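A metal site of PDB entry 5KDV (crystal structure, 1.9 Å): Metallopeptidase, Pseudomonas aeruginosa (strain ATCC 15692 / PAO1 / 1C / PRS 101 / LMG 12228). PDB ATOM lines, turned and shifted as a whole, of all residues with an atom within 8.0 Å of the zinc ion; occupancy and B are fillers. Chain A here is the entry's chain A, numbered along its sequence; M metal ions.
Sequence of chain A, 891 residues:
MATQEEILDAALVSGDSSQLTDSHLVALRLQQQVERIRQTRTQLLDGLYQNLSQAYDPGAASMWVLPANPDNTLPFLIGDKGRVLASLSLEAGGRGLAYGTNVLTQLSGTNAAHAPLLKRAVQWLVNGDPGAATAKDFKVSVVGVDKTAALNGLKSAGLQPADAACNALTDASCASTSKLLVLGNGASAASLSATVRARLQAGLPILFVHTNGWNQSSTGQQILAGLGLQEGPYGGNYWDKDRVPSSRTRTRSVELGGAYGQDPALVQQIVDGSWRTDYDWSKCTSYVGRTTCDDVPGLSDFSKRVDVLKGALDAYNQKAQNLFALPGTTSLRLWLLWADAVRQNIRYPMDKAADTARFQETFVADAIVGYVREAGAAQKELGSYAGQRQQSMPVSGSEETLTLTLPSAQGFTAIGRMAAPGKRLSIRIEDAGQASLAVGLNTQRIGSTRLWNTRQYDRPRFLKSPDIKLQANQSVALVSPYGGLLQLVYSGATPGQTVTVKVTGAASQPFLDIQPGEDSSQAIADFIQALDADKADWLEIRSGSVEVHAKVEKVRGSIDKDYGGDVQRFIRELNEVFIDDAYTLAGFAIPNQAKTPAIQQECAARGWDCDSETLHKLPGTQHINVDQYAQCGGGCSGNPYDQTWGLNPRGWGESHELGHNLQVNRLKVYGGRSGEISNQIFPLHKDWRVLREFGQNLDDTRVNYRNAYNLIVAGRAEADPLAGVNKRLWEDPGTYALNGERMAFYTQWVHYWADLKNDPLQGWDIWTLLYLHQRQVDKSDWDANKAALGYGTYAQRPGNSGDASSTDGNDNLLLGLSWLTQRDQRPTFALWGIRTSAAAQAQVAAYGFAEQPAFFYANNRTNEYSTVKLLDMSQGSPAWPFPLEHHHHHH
O of His 656 lies within hydrogen-bond range of ND2 of Asn 679, at 3.0 Å.
OE1 of Gln 680 lies within hydrogen-bond range of ND1 of His 656, at 2.8 Å.
ND1 of His 660 sits close to ND2 of Asn 679, at 3.5 Å.
The backbone carbonyl oxygen of Glu 676 is in hydrogen-bond range of the side-chain amide nitrogen of Asn 739.
The backbone carbonyl oxygen (O) of Glu 676 sits close to the side-chain amide nitrogen (NE2) of Gln 680 (3.4 Å).
A ring nitrogen (ND1) of His 660 lies within hydrogen-bond range of the side-chain amide oxygen (OE1) of Gln 663, at 2.8 Å.
Glu 657 touches the zinc ion.
The side-chain carboxylate (OE1) of Glu 676 binds the zinc ion (2.0 Å).
A ring nitrogen (NE2) of His 656 binds the zinc ion (2.1 Å).
The zinc ion is bound by a ring nitrogen (NE2) of His 660 (2.1 Å).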
ATOM      1  N   SER A 637     -13.397  -3.913  -6.489  1.00  0.00           N
ATOM      2  CA  SER A 637     -13.499  -5.046  -7.371  1.00  0.00           C
ATOM      3  C   SER A 637     -14.755  -4.979  -8.204  1.00  0.00           C
ATOM      4  O   SER A 637     -15.695  -4.287  -7.825  1.00  0.00           O
ATOM      5  CB  SER A 637     -13.492  -6.344  -6.540  1.00  0.00           C
ATOM      6  OG  SER A 637     -14.656  -6.442  -5.729  1.00  0.00           O
ATOM      7  N   TRP A 652       0.637  -3.107  -8.889  1.00  0.00           N
ATOM      8  CA  TRP A 652       0.279  -4.412  -8.364  1.00  0.00           C
ATOM      9  C   TRP A 652      -1.237  -4.653  -8.437  1.00  0.00           C
ATOM     10  O   TRP A 652      -1.706  -5.671  -8.978  1.00  0.00           O
ATOM     11  CB  TRP A 652       0.772  -4.535  -6.922  1.00  0.00           C
ATOM     12  CG  TRP A 652       0.407  -5.841  -6.326  1.00  0.00           C
ATOM     13  CD1 TRP A 652      -0.781  -6.149  -5.700  1.00  0.00           C
ATOM     14  CD2 TRP A 652       1.187  -7.017  -6.307  1.00  0.00           C
ATOM     15  NE1 TRP A 652      -0.757  -7.433  -5.287  1.00  0.00           N
ATOM     16  CE2 TRP A 652       0.443  -7.998  -5.635  1.00  0.00           C
ATOM     17  CE3 TRP A 652       2.476  -7.350  -6.790  1.00  0.00           C
ATOM     18  CZ2 TRP A 652       0.924  -9.309  -5.452  1.00  0.00           C
ATOM     19  CZ3 TRP A 652       2.947  -8.641  -6.624  1.00  0.00           C
ATOM     20  CH2 TRP A 652       2.168  -9.621  -5.989  1.00  0.00           C
ATOM     21  N   GLY A 653      -1.998  -3.689  -7.943  1.00  0.00           N
ATOM     22  CA  GLY A 653      -3.458  -3.776  -7.880  1.00  0.00           C
ATOM     23  C   GLY A 653      -4.044  -4.040  -9.261  1.00  0.00           C
ATOM     24  O   GLY A 653      -4.923  -4.914  -9.413  1.00  0.00           O
ATOM     25  N   HIS A 656      -3.434  -7.694 -10.134  1.00  0.00           N
ATOM     26  CA  HIS A 656      -4.116  -8.541  -9.156  1.00  0.00           C
ATOM     27  C   HIS A 656      -5.586  -8.625  -9.508  1.00  0.00           C
ATOM     28  O   HIS A 656      -6.165  -9.714  -9.578  1.00  0.00           O
ATOM     29  CB  HIS A 656      -3.962  -7.926  -7.755  1.00  0.00           C
ATOM     30  CG  HIS A 656      -4.781  -8.589  -6.707  1.00  0.00           C
ATOM     31  ND1 HIS A 656      -4.259  -9.530  -5.841  1.00  0.00           N
ATOM     32  CD2 HIS A 656      -6.057  -8.385  -6.325  1.00  0.00           C
ATOM     33  CE1 HIS A 656      -5.196  -9.909  -4.997  1.00  0.00           C
ATOM     34  NE2 HIS A 656      -6.299  -9.237  -5.278  1.00  0.00           N
ATOM     35  N   GLU A 657      -6.159  -7.477  -9.785  1.00  0.00           N
ATOM     36  CA  GLU A 657      -7.578  -7.432 -10.073  1.00  0.00           C
ATOM     37  C   GLU A 657      -7.962  -7.950 -11.457  1.00  0.00           C
ATOM     38  O   GLU A 657      -9.003  -8.672 -11.586  1.00  0.00           O
ATOM     39  CB  GLU A 657      -8.119  -6.032  -9.845  1.00  0.00           C
ATOM     40  CG  GLU A 657      -9.535  -6.005  -9.386  1.00  0.00           C
ATOM     41  CD  GLU A 657      -9.762  -6.686  -8.045  1.00  0.00           C
ATOM     42  OE1 GLU A 657      -8.887  -6.749  -7.152  1.00  0.00           O
ATOM     43  OE2 GLU A 657     -10.883  -7.167  -7.876  1.00  0.00           O
ATOM     44  N   GLY A 659      -6.235 -10.240 -12.747  1.00  0.00           N
ATOM     45  CA  GLY A 659      -6.073 -11.632 -12.407  1.00  0.00           C
ATOM     46  C   GLY A 659      -7.300 -12.341 -11.882  1.00  0.00           C
ATOM     47  O   GLY A 659      -7.526 -13.518 -12.232  1.00  0.00           O
ATOM     48  N   HIS A 660      -8.082 -11.671 -11.040  1.00  0.00           N
ATOM     49  CA  HIS A 660      -9.365 -12.240 -10.678  1.00  0.00           C
ATOM     50  C   HIS A 660     -10.273 -12.640 -11.849  1.00  0.00           C
ATOM     51  O   HIS A 660     -10.888 -13.711 -11.833  1.00  0.00           O
ATOM     52  CB  HIS A 660     -10.137 -11.308  -9.779  1.00  0.00           C
ATOM     53  CG  HIS A 660      -9.662 -11.297  -8.390  1.00  0.00           C
ATOM     54  ND1 HIS A 660      -9.425 -12.434  -7.667  1.00  0.00           N
ATOM     55  CD2 HIS A 660      -9.448 -10.257  -7.538  1.00  0.00           C
ATOM     56  CE1 HIS A 660      -9.031 -12.111  -6.448  1.00  0.00           C
ATOM     57  NE2 HIS A 660      -9.059 -10.790  -6.356  1.00  0.00           N
ATOM     58  N   GLN A 663      -9.070 -16.087 -13.237  1.00  0.00           N
ATOM     59  CA  GLN A 663      -8.963 -17.266 -12.425  1.00  0.00           C
ATOM     60  C   GLN A 663      -9.859 -18.382 -12.941  1.00  0.00           C
ATOM     61  O   GLN A 663     -10.926 -18.118 -13.508  1.00  0.00           O
ATOM     62  CB  GLN A 663      -9.336 -16.948 -10.948  1.00  0.00           C
ATOM     63  CG  GLN A 663      -8.173 -16.318 -10.187  1.00  0.00           C
ATOM     64  CD  GLN A 663      -8.611 -15.782  -8.834  1.00  0.00           C
ATOM     65  OE1 GLN A 663      -9.537 -14.981  -8.740  1.00  0.00           O
ATOM     66  NE2 GLN A 663      -7.970 -16.262  -7.773  1.00  0.00           N
ATOM     67  N   GLY A 675      -8.435 -18.101  -3.400  1.00  0.00           N
ATOM     68  CA  GLY A 675      -9.247 -17.061  -4.087  1.00  0.00           C
ATOM     69  C   GLY A 675      -8.456 -15.714  -4.199  1.00  0.00           C
ATOM     70  O   GLY A 675      -8.687 -14.961  -5.130  1.00  0.00           O
ATOM     71  N   GLU A 676      -7.494 -15.475  -3.314  1.00  0.00           N
ATOM     72  CA  GLU A 676      -6.595 -14.298  -3.394  1.00  0.00           C
ATOM     73  C   GLU A 676      -5.160 -14.719  -3.667  1.00  0.00           C
ATOM     74  O   GLU A 676      -4.184 -13.970  -3.401  1.00  0.00           O
ATOM     75  CB  GLU A 676      -6.672 -13.496  -2.089  1.00  0.00           C
ATOM     76  CG  GLU A 676      -8.079 -12.977  -1.843  1.00  0.00           C
ATOM     77  CD  GLU A 676      -8.464 -11.873  -2.801  1.00  0.00           C
ATOM     78  OE1 GLU A 676      -7.613 -11.272  -3.535  1.00  0.00           O
ATOM     79  OE2 GLU A 676      -9.664 -11.610  -2.861  1.00  0.00           O
ATOM     80  N   ILE A 677      -4.992 -15.931  -4.188  1.00  0.00           N
ATOM     81  CA  ILE A 677      -3.656 -16.459  -4.428  1.00  0.00           C
ATOM     82  C   ILE A 677      -3.413 -16.768  -5.905  1.00  0.00           C
ATOM     83  O   ILE A 677      -2.410 -16.360  -6.511  1.00  0.00           O
ATOM     84  CB  ILE A 677      -3.397 -17.741  -3.599  1.00  0.00           C
ATOM     85  CG1 ILE A 677      -3.616 -17.536  -2.083  1.00  0.00           C
ATOM     86  CG2 ILE A 677      -2.020 -18.269  -3.873  1.00  0.00           C
ATOM     87  CD1 ILE A 677      -2.636 -16.570  -1.441  1.00  0.00           C
ATOM     88  N   ASN A 679      -4.788 -15.786  -8.586  1.00  0.00           N
ATOM     89  CA  ASN A 679      -4.664 -14.566  -9.406  1.00  0.00           C
ATOM     90  C   ASN A 679      -3.316 -13.819  -9.297  1.00  0.00           C
ATOM     91  O   ASN A 679      -3.012 -12.950 -10.149  1.00  0.00           O
ATOM     92  CB  ASN A 679      -5.798 -13.643  -9.102  1.00  0.00           C
ATOM     93  CG  ASN A 679      -5.807 -13.130  -7.675  1.00  0.00           C
ATOM     94  OD1 ASN A 679      -5.677 -13.896  -6.716  1.00  0.00           O
ATOM     95  ND2 ASN A 679      -5.998 -11.843  -7.524  1.00  0.00           N
ATOM     96  N   GLN A 680      -2.525 -14.146  -8.252  1.00  0.00           N
ATOM     97  CA  GLN A 680      -1.299 -13.435  -7.936  1.00  0.00           C
ATOM     98  C   GLN A 680      -0.192 -13.750  -8.931  1.00  0.00           C
ATOM     99  O   GLN A 680       0.776 -13.009  -9.015  1.00  0.00           O
ATOM    100  CB  GLN A 680      -0.789 -13.740  -6.520  1.00  0.00           C
ATOM    101  CG  GLN A 680      -1.742 -13.389  -5.405  1.00  0.00           C
ATOM    102  CD  GLN A 680      -1.843 -11.915  -5.155  1.00  0.00           C
ATOM    103  OE1 GLN A 680      -1.986 -11.121  -6.096  1.00  0.00           O
ATOM    104  NE2 GLN A 680      -1.850 -11.519  -3.853  1.00  0.00           N
ATOM    105  N   THR A 735      -9.840 -13.793   4.425  1.00  0.00           N
ATOM    106  CA  THR A 735      -9.750 -13.418   3.009  1.00  0.00           C
ATOM    107  C   THR A 735      -8.312 -13.359   2.478  1.00  0.00           C
ATOM    108  O   THR A 735      -8.038 -13.880   1.415  1.00  0.00           O
ATOM    109  CB  THR A 735     -10.376 -12.059   2.777  1.00  0.00           C
ATOM    110  OG1 THR A 735     -11.685 -12.028   3.355  1.00  0.00           O
ATOM    111  CG2 THR A 735     -10.458 -11.731   1.295  1.00  0.00           C
ATOM    112  N   TYR A 736      -7.419 -12.705   3.193  1.00  0.00           N
ATOM    113  CA  TYR A 736      -5.988 -12.649   2.777  1.00  0.00           C
ATOM    114  C   TYR A 736      -5.123 -13.425   3.719  1.00  0.00           C
ATOM    115  O   TYR A 736      -3.940 -13.145   3.811  1.00  0.00           O
ATOM    116  CB  TYR A 736      -5.452 -11.216   2.627  1.00  0.00           C
ATOM    117  CG  TYR A 736      -6.245 -10.430   1.635  1.00  0.00           C
ATOM    118  CD1 TYR A 736      -5.898 -10.368   0.303  1.00  0.00           C
ATOM    119  CD2 TYR A 736      -7.328  -9.727   2.068  1.00  0.00           C
ATOM    120  CE1 TYR A 736      -6.666  -9.621  -0.587  1.00  0.00           C
ATOM    121  CE2 TYR A 736      -8.083  -8.979   1.217  1.00  0.00           C
ATOM    122  CZ  TYR A 736      -7.787  -8.951  -0.103  1.00  0.00           C
ATOM    123  OH  TYR A 736      -8.627  -8.181  -0.836  1.00  0.00           O
ATOM    124  N   ASN A 739      -1.320 -14.961   2.866  1.00  0.00           N
ATOM    125  CA  ASN A 739      -1.298 -14.666   1.452  1.00  0.00           C
ATOM    126  C   ASN A 739       0.109 -14.869   0.897  1.00  0.00           C
ATOM    127  O   ASN A 739       0.319 -15.486  -0.162  1.00  0.00           O
ATOM    128  CB  ASN A 739      -1.730 -13.219   1.217  1.00  0.00           C
ATOM    129  CG  ASN A 739      -2.159 -12.986  -0.200  1.00  0.00           C
ATOM    130  OD1 ASN A 739      -1.385 -12.509  -1.026  1.00  0.00           O
ATOM    131  ND2 ASN A 739      -3.403 -13.338  -0.491  1.00  0.00           N
HETATM  132 ZN    ZN M   1      -8.278  -9.749  -4.660  1.00  0.00          ZN
